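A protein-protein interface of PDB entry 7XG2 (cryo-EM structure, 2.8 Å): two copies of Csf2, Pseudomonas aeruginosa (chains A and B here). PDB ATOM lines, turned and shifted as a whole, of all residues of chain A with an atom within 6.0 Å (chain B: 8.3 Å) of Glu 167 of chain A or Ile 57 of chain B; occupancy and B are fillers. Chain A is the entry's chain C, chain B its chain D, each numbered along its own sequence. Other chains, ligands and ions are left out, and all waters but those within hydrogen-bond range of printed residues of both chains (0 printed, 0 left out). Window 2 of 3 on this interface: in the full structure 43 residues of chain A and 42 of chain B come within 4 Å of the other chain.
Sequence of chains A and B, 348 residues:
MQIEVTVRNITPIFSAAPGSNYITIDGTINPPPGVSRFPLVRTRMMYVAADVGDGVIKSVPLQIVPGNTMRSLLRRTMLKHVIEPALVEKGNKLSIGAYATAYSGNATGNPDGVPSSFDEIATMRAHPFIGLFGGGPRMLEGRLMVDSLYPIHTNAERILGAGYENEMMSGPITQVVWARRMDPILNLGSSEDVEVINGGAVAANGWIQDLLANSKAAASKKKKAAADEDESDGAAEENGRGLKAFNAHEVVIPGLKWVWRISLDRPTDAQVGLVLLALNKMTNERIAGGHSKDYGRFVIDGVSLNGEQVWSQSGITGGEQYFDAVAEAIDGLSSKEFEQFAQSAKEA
The guanidinium group of Arg 158 of chain B lies within salt-bridge range of the side-chain carboxylate of Glu 167 of chain A (3.0 Å).
The backbone NH (N) of Ser 59 of chain B sits at hydrogen-bond distance from the side-chain sulfur (SD) of Met 169 of chain A, at 3.7 Å.
The guanidinium group (NE) of Arg 158 of chain B is in hydrogen-bond range of the backbone carbonyl oxygen (O) of Gly 255 of chain A (2.6 Å).
The side-chain sulfur (SD) of Met 169 of chain A sits close to the backbone carbonyl oxygen (O) of Ile 57 of chain B (3.6 Å).
O of Ile 152 of chain A sits at hydrogen-bond distance from N of Met 169 of chain A, 2.9 Å away.
O of Lys 257 of chain A lies within hydrogen-bond range of N of Ile 152 of chain A, at 2.6 Å.
The side-chain amino group (NZ) of Lys 257 of chain A lies within salt-bridge range of the side-chain carboxylate (OE2) of Glu 167 of chain A (3.9 Å).
The side-chain amino group of Lys 257 of chain A is in salt-bridge range of the side-chain carboxylate of Asp 301 of chain A, 2.7 Å away.
The backbone carbonyl oxygen (O) of Ala 49 of chain B sits close to the guanidinium group (NE) of Arg 158 of chain B (3.5 Å).
The backbone NH of Ala 50 of chain B is in hydrogen-bond range of the backbone carbonyl oxygen of Lys 58 of chain B.
Among the printed residues, merely in contact across the chains: Glu 167 of chain A with Ile 57 of chain B, Met 169 of chain A with Ala 49 of chain B, Met 169 of chain A with Lys 58 of chain B, Gly 255 of chain A with Ala 49 of chain B, Leu 256 of chain A with Ala 49 of chain B, Leu 256 of chain A with Arg 158 of chain B and Lys 257 of chain A with Arg 158 of chain B.
Of the printed residues of chain B, Glu 167 of chain A touches Ile 57 (3.9 Å) and Arg 158 (3.0 Å).
Of chain A, only Glu 167 (3.9 Å) and Met 169 (3.6 Å) come within 4 Å of Ile 57 of chain B.
Printed residues of chain A within 4 Å of Ser 59 of chain B: Met 169.
Of the printed residues of chain B, Met 169 of chain A touches Ala 49, Ile 57, Lys 58 and Ser 59.
The nearest printed residue of chain B that does not touch Leu 256 of chain A is Ile 57 of chain B (5.9 Å).
Of the 13 printed residues of chain A, 5 touch a printed residue of chain B.
Hydrophobic or aromatic side chains of chain A within 4 Å of the printed part of chain B: Met 169 and Leu 256.
Printed residues of chain B that touch a printed residue of chain A: Ala 49, Ile 57, Lys 58, Ser 59 and Arg 158.
Among the printed residues, Asp or Glu carboxylates within 4 Å of a Lys or Arg side-chain nitrogen of the other chain: Glu 167 of chain A with Arg 158 of chain B (3.0 Å).
No position is printed for both chains.
Of the 11 pairs that touch across the chains among the printed residues, none has its exchanged pair printed and touching as well.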
ATOM      1  N   ILE A 152      15.039  25.077  15.866  1.00  0.00           N
ATOM      2  CA  ILE A 152      15.820  24.640  14.720  1.00  0.00           C
ATOM      3  C   ILE A 152      15.202  23.328  14.266  1.00  0.00           C
ATOM      4  O   ILE A 152      15.490  22.257  14.810  1.00  0.00           O
ATOM      5  CB  ILE A 152      17.317  24.510  15.044  1.00  0.00           C
ATOM      6  CG1 ILE A 152      17.859  25.865  15.501  1.00  0.00           C
ATOM      7  CG2 ILE A 152      18.076  24.045  13.815  1.00  0.00           C
ATOM      8  CD1 ILE A 152      19.358  25.914  15.684  1.00  0.00           C
ATOM      9  N   HIS A 153      14.324  23.428  13.275  1.00  0.00           N
ATOM     10  CA  HIS A 153      13.415  22.370  12.884  1.00  0.00           C
ATOM     11  C   HIS A 153      13.168  22.496  11.391  1.00  0.00           C
ATOM     12  O   HIS A 153      13.280  23.588  10.830  1.00  0.00           O
ATOM     13  CB  HIS A 153      12.101  22.481  13.667  1.00  0.00           C
ATOM     14  CG  HIS A 153      11.228  21.270  13.581  1.00  0.00           C
ATOM     15  ND1 HIS A 153      10.145  21.196  12.732  1.00  0.00           N
ATOM     16  CD2 HIS A 153      11.261  20.095  14.252  1.00  0.00           C
ATOM     17  CE1 HIS A 153       9.555  20.024  12.877  1.00  0.00           C
ATOM     18  NE2 HIS A 153      10.212  19.338  13.793  1.00  0.00           N
ATOM     19  N   TYR A 164      21.629  25.945   8.997  1.00  0.00           N
ATOM     20  CA  TYR A 164      21.040  25.283  10.152  1.00  0.00           C
ATOM     21  C   TYR A 164      20.604  23.855   9.854  1.00  0.00           C
ATOM     22  O   TYR A 164      19.818  23.293  10.626  1.00  0.00           O
ATOM     23  CB  TYR A 164      19.839  26.075  10.680  1.00  0.00           C
ATOM     24  CG  TYR A 164      20.191  27.433  11.231  1.00  0.00           C
ATOM     25  CD1 TYR A 164      20.906  27.560  12.415  1.00  0.00           C
ATOM     26  CD2 TYR A 164      19.804  28.589  10.569  1.00  0.00           C
ATOM     27  CE1 TYR A 164      21.230  28.802  12.921  1.00  0.00           C
ATOM     28  CE2 TYR A 164      20.118  29.832  11.066  1.00  0.00           C
ATOM     29  CZ  TYR A 164      20.831  29.933  12.240  1.00  0.00           C
ATOM     30  OH  TYR A 164      21.145  31.173  12.731  1.00  0.00           O
ATOM     31  N   GLU A 165      21.085  23.256   8.761  1.00  0.00           N
ATOM     32  CA  GLU A 165      20.676  21.899   8.414  1.00  0.00           C
ATOM     33  C   GLU A 165      21.247  20.873   9.383  1.00  0.00           C
ATOM     34  O   GLU A 165      20.609  19.848   9.647  1.00  0.00           O
ATOM     35  CB  GLU A 165      21.086  21.578   6.976  1.00  0.00           C
ATOM     36  CG  GLU A 165      20.046  21.957   5.917  1.00  0.00           C
ATOM     37  CD  GLU A 165      20.135  23.404   5.439  1.00  0.00           C
ATOM     38  OE1 GLU A 165      20.546  24.295   6.213  1.00  0.00           O
ATOM     39  OE2 GLU A 165      19.782  23.654   4.267  1.00  0.00           O
ATOM     40  N   ASN A 166      22.439  21.123   9.916  1.00  0.00           N
ATOM     41  CA  ASN A 166      22.921  20.334  11.039  1.00  0.00           C
ATOM     42  C   ASN A 166      22.174  20.730  12.307  1.00  0.00           C
ATOM     43  O   ASN A 166      21.762  21.885  12.458  1.00  0.00           O
ATOM     44  CB  ASN A 166      24.437  20.502  11.199  1.00  0.00           C
ATOM     45  CG  ASN A 166      24.868  21.955  11.394  1.00  0.00           C
ATOM     46  OD1 ASN A 166      24.582  22.585  12.413  1.00  0.00           O
ATOM     47  ND2 ASN A 166      25.563  22.491  10.398  1.00  0.00           N
ATOM     48  N   GLU A 167      21.992  19.751  13.203  1.00  0.00           N
ATOM     49  CA  GLU A 167      21.236  19.886  14.457  1.00  0.00           C
ATOM     50  C   GLU A 167      19.805  20.372  14.219  1.00  0.00           C
ATOM     51  O   GLU A 167      19.257  21.144  15.010  1.00  0.00           O
ATOM     52  CB  GLU A 167      21.958  20.799  15.456  1.00  0.00           C
ATOM     53  CG  GLU A 167      21.902  20.325  16.893  1.00  0.00           C
ATOM     54  CD  GLU A 167      23.068  20.842  17.709  1.00  0.00           C
ATOM     55  OE1 GLU A 167      23.449  22.016  17.522  1.00  0.00           O
ATOM     56  OE2 GLU A 167      23.606  20.076  18.536  1.00  0.00           O
ATOM     57  N   MET A 168      19.191  19.916  13.133  1.00  0.00           N
ATOM     58  CA  MET A 168      17.838  20.313  12.755  1.00  0.00           C
ATOM     59  C   MET A 168      16.903  19.186  13.170  1.00  0.00           C
ATOM     60  O   MET A 168      16.999  18.069  12.658  1.00  0.00           O
ATOM     61  CB  MET A 168      17.755  20.573  11.256  1.00  0.00           C
ATOM     62  CG  MET A 168      16.674  21.543  10.830  1.00  0.00           C
ATOM     63  SD  MET A 168      17.085  22.244   9.222  1.00  0.00           S
ATOM     64  CE  MET A 168      16.122  23.743   9.220  1.00  0.00           C
ATOM     65  N   MET A 169      15.998  19.476  14.101  1.00  0.00           N
ATOM     66  CA  MET A 169      15.060  18.462  14.566  1.00  0.00           C
ATOM     67  C   MET A 169      13.984  18.231  13.514  1.00  0.00           C
ATOM     68  O   MET A 169      13.799  19.062  12.622  1.00  0.00           O
ATOM     69  CB  MET A 169      14.433  18.874  15.898  1.00  0.00           C
ATOM     70  CG  MET A 169      14.989  18.122  17.093  1.00  0.00           C
ATOM     71  SD  MET A 169      14.242  16.501  17.319  1.00  0.00           S
ATOM     72  CE  MET A 169      12.634  16.952  17.951  1.00  0.00           C
ATOM     73  N   SER A 170      13.274  17.110  13.599  1.00  0.00           N
ATOM     74  CA  SER A 170      12.226  16.811  12.636  1.00  0.00           C
ATOM     75  C   SER A 170      11.096  16.079  13.341  1.00  0.00           C
ATOM     76  O   SER A 170      11.266  15.526  14.430  1.00  0.00           O
ATOM     77  CB  SER A 170      12.760  15.989  11.459  1.00  0.00           C
ATOM     78  OG  SER A 170      11.878  16.058  10.353  1.00  0.00           O
ATOM     79  N   GLY A 255      15.435  19.970  25.390  1.00  0.00           N
ATOM     80  CA  GLY A 255      16.672  19.534  24.783  1.00  0.00           C
ATOM     81  C   GLY A 255      16.913  19.999  23.367  1.00  0.00           C
ATOM     82  O   GLY A 255      18.020  19.795  22.854  1.00  0.00           O
ATOM     83  N   LEU A 256      15.938  20.620  22.715  1.00  0.00           N
ATOM     84  CA  LEU A 256      16.110  21.028  21.330  1.00  0.00           C
ATOM     85  C   LEU A 256      16.706  22.427  21.253  1.00  0.00           C
ATOM     86  O   LEU A 256      16.901  23.110  22.258  1.00  0.00           O
ATOM     87  CB  LEU A 256      14.785  20.943  20.562  1.00  0.00           C
ATOM     88  CG  LEU A 256      13.572  21.812  20.874  1.00  0.00           C
ATOM     89  CD1 LEU A 256      13.534  23.029  19.989  1.00  0.00           C
ATOM     90  CD2 LEU A 256      12.330  20.994  20.655  1.00  0.00           C
ATOM     91  N   LYS A 257      16.985  22.853  20.026  1.00  0.00           N
ATOM     92  CA  LYS A 257      17.741  24.066  19.766  1.00  0.00           C
ATOM     93  C   LYS A 257      16.868  25.099  19.067  1.00  0.00           C
ATOM     94  O   LYS A 257      16.044  24.758  18.214  1.00  0.00           O
ATOM     95  CB  LYS A 257      18.972  23.751  18.920  1.00  0.00           C
ATOM     96  CG  LYS A 257      20.110  24.712  19.125  1.00  0.00           C
ATOM     97  CD  LYS A 257      20.968  24.314  20.310  1.00  0.00           C
ATOM     98  CE  LYS A 257      21.573  22.941  20.119  1.00  0.00           C
ATOM     99  NZ  LYS A 257      22.392  22.521  21.286  1.00  0.00           N
ATOM    100  N   ASP A 301      23.627  28.716  23.740  1.00  0.00           N
ATOM    101  CA  ASP A 301      24.687  27.948  23.105  1.00  0.00           C
ATOM    102  C   ASP A 301      25.549  28.772  22.164  1.00  0.00           C
ATOM    103  O   ASP A 301      26.725  28.445  21.979  1.00  0.00           O
ATOM    104  CB  ASP A 301      24.093  26.762  22.338  1.00  0.00           C
ATOM    105  CG  ASP A 301      23.922  25.535  23.211  1.00  0.00           C
ATOM    106  OD1 ASP A 301      24.577  25.462  24.272  1.00  0.00           O
ATOM    107  OD2 ASP A 301      23.140  24.641  22.834  1.00  0.00           O
ATOM    108  N   VAL B  48      12.138  13.867  24.202  1.00  0.00           N
ATOM    109  CA  VAL B  48      13.285  14.750  24.348  1.00  0.00           C
ATOM    110  C   VAL B  48      14.109  14.694  23.068  1.00  0.00           C
ATOM    111  O   VAL B  48      14.312  13.619  22.496  1.00  0.00           O
ATOM    112  CB  VAL B  48      14.117  14.379  25.601  1.00  0.00           C
ATOM    113  CG1 VAL B  48      14.425  12.892  25.647  1.00  0.00           C
ATOM    114  CG2 VAL B  48      15.396  15.188  25.688  1.00  0.00           C
ATOM    115  N   ALA B  49      14.526  15.859  22.584  1.00  0.00           N
ATOM    116  CA  ALA B  49      15.499  15.911  21.504  1.00  0.00           C
ATOM    117  C   ALA B  49      16.846  15.450  22.044  1.00  0.00           C
ATOM    118  O   ALA B  49      17.372  16.030  22.999  1.00  0.00           O
ATOM    119  CB  ALA B  49      15.592  17.319  20.928  1.00  0.00           C
ATOM    120  N   ALA B  50      17.390  14.396  21.448  1.00  0.00           N
ATOM    121  CA  ALA B  50      18.632  13.799  21.902  1.00  0.00           C
ATOM    122  C   ALA B  50      19.521  13.485  20.711  1.00  0.00           C
ATOM    123  O   ALA B  50      19.070  13.424  19.563  1.00  0.00           O
ATOM    124  CB  ALA B  50      18.385  12.524  22.707  1.00  0.00           C
ATOM    125  N   ASP B  51      20.799  13.271  21.015  1.00  0.00           N
ATOM    126  CA  ASP B  51      21.825  13.043  20.003  1.00  0.00           C
ATOM    127  C   ASP B  51      21.959  11.532  19.852  1.00  0.00           C
ATOM    128  O   ASP B  51      22.620  10.869  20.655  1.00  0.00           O
ATOM    129  CB  ASP B  51      23.126  13.728  20.427  1.00  0.00           C
ATOM    130  CG  ASP B  51      24.254  13.638  19.383  1.00  0.00           C
ATOM    131  OD1 ASP B  51      24.543  12.569  18.811  1.00  0.00           O
ATOM    132  OD2 ASP B  51      24.906  14.680  19.165  1.00  0.00           O
ATOM    133  N   VAL B  52      21.326  10.986  18.819  1.00  0.00           N
ATOM    134  CA  VAL B  52      21.523   9.598  18.419  1.00  0.00           C
ATOM    135  C   VAL B  52      22.335   9.596  17.128  1.00  0.00           C
ATOM    136  O   VAL B  52      22.014  10.313  16.173  1.00  0.00           O
ATOM    137  CB  VAL B  52      20.182   8.852  18.283  1.00  0.00           C
ATOM    138  CG1 VAL B  52      19.157   9.643  17.466  1.00  0.00           C
ATOM    139  CG2 VAL B  52      20.394   7.464  17.690  1.00  0.00           C
ATOM    140  N   GLY B  53      23.424   8.838  17.114  1.00  0.00           N
ATOM    141  CA  GLY B  53      24.349   8.911  15.993  1.00  0.00           C
ATOM    142  C   GLY B  53      25.206  10.152  16.106  1.00  0.00           C
ATOM    143  O   GLY B  53      25.686  10.485  17.191  1.00  0.00           O
ATOM    144  N   ASP B  54      25.401  10.844  14.986  1.00  0.00           N
ATOM    145  CA  ASP B  54      26.187  12.078  14.935  1.00  0.00           C
ATOM    146  C   ASP B  54      25.334  13.171  14.297  1.00  0.00           C
ATOM    147  O   ASP B  54      25.212  13.228  13.070  1.00  0.00           O
ATOM    148  CB  ASP B  54      27.486  11.874  14.157  1.00  0.00           C
ATOM    149  CG  ASP B  54      28.504  11.045  14.919  1.00  0.00           C
ATOM    150  OD1 ASP B  54      28.348  10.878  16.146  1.00  0.00           O
ATOM    151  OD2 ASP B  54      29.464  10.559  14.286  1.00  0.00           O
ATOM    152  N   GLY B  55      24.759  14.042  15.125  1.00  0.00           N
ATOM    153  CA  GLY B  55      23.949  15.140  14.638  1.00  0.00           C
ATOM    154  C   GLY B  55      22.639  14.746  13.994  1.00  0.00           C
ATOM    155  O   GLY B  55      22.151  15.475  13.124  1.00  0.00           O
ATOM    156  N   VAL B  56      22.056  13.619  14.391  1.00  0.00           N
ATOM    157  CA  VAL B  56      20.837  13.092  13.790  1.00  0.00           C
ATOM    158  C   VAL B  56      19.762  13.228  14.865  1.00  0.00           C
ATOM    159  O   VAL B  56      18.989  12.293  15.107  1.00  0.00           O
ATOM    160  CB  VAL B  56      21.018  11.641  13.293  1.00  0.00           C
ATOM    161  CG1 VAL B  56      19.946  11.255  12.253  1.00  0.00           C
ATOM    162  CG2 VAL B  56      22.412  11.432  12.730  1.00  0.00           C
ATOM    163  N   ILE B  57      19.813  14.358  15.589  1.00  0.00           N
ATOM    164  CA  ILE B  57      19.003  14.717  16.759  1.00  0.00           C
ATOM    165  C   ILE B  57      17.529  14.374  16.581  1.00  0.00           C
ATOM    166  O   ILE B  57      16.885  14.817  15.623  1.00  0.00           O
ATOM    167  CB  ILE B  57      19.143  16.222  17.064  1.00  0.00           C
ATOM    168  CG1 ILE B  57      20.594  16.691  16.921  1.00  0.00           C
ATOM    169  CG2 ILE B  57      18.607  16.544  18.448  1.00  0.00           C
ATOM    170  CD1 ILE B  57      21.540  16.120  17.938  1.00  0.00           C
ATOM    171  N   LYS B  58      16.987  13.588  17.508  1.00  0.00           N
ATOM    172  CA  LYS B  58      15.675  12.989  17.328  1.00  0.00           C
ATOM    173  C   LYS B  58      14.888  13.078  18.626  1.00  0.00           C
ATOM    174  O   LYS B  58      15.457  13.150  19.717  1.00  0.00           O
ATOM    175  CB  LYS B  58      15.787  11.524  16.883  1.00  0.00           C
ATOM    176  CG  LYS B  58      15.695  11.317  15.383  1.00  0.00           C
ATOM    177  CD  LYS B  58      14.258  11.403  14.897  1.00  0.00           C
ATOM    178  CE  LYS B  58      14.091  10.709  13.558  1.00  0.00           C
ATOM    179  NZ  LYS B  58      15.004  11.275  12.528  1.00  0.00           N
ATOM    180  N   SER B  59      13.566  13.075  18.492  1.00  0.00           N
ATOM    181  CA  SER B  59      12.667  13.061  19.643  1.00  0.00           C
ATOM    182  C   SER B  59      12.534  11.624  20.127  1.00  0.00           C
ATOM    183  O   SER B  59      11.804  10.821  19.541  1.00  0.00           O
ATOM    184  CB  SER B  59      11.313  13.653  19.273  1.00  0.00           C
ATOM    185  OG  SER B  59      10.297  13.180  20.137  1.00  0.00           O
ATOM    186  N   VAL B  60      13.241  11.294  21.202  1.00  0.00           N
ATOM    187  CA  VAL B  60      13.222   9.943  21.754  1.00  0.00           C
ATOM    188  C   VAL B  60      12.494   9.944  23.094  1.00  0.00           C
ATOM    189  O   VAL B  60      12.422  10.985  23.764  1.00  0.00           O
ATOM    190  CB  VAL B  60      14.644   9.379  21.893  1.00  0.00           C
ATOM    191  CG1 VAL B  60      15.315   9.306  20.533  1.00  0.00           C
ATOM    192  CG2 VAL B  60      15.467  10.223  22.845  1.00  0.00           C
ATOM    193  N   GLU B 157      21.121  14.001  27.431  1.00  0.00           N
ATOM    194  CA  GLU B 157      22.475  14.554  27.383  1.00  0.00           C
ATOM    195  C   GLU B 157      22.470  16.044  27.052  1.00  0.00           C
ATOM    196  O   GLU B 157      23.278  16.809  27.591  1.00  0.00           O
ATOM    197  CB  GLU B 157      23.311  13.773  26.365  1.00  0.00           C
ATOM    198  CG  GLU B 157      24.750  14.250  26.189  1.00  0.00           C
ATOM    199  CD  GLU B 157      24.924  15.176  24.995  1.00  0.00           C
ATOM    200  OE1 GLU B 157      24.760  14.709  23.848  1.00  0.00           O
ATOM    201  OE2 GLU B 157      25.216  16.372  25.206  1.00  0.00           O
ATOM    202  N   ARG B 158      21.556  16.474  26.181  1.00  0.00           N
ATOM    203  CA  ARG B 158      21.441  17.894  25.866  1.00  0.00           C
ATOM    204  C   ARG B 158      20.882  18.676  27.048  1.00  0.00           C
ATOM    205  O   ARG B 158      21.183  19.862  27.222  1.00  0.00           O
ATOM    206  CB  ARG B 158      20.567  18.088  24.629  1.00  0.00           C
ATOM    207  CG  ARG B 158      21.292  17.846  23.324  1.00  0.00           C
ATOM    208  CD  ARG B 158      20.365  17.258  22.272  1.00  0.00           C
ATOM    209  NE  ARG B 158      19.614  18.277  21.547  1.00  0.00           N
ATOM    210  CZ  ARG B 158      20.113  19.076  20.612  1.00  0.00           C
ATOM    211  NH1 ARG B 158      21.373  18.982  20.217  1.00  0.00           N
ATOM    212  NH2 ARG B 158      19.323  19.985  20.049  1.00  0.00           N
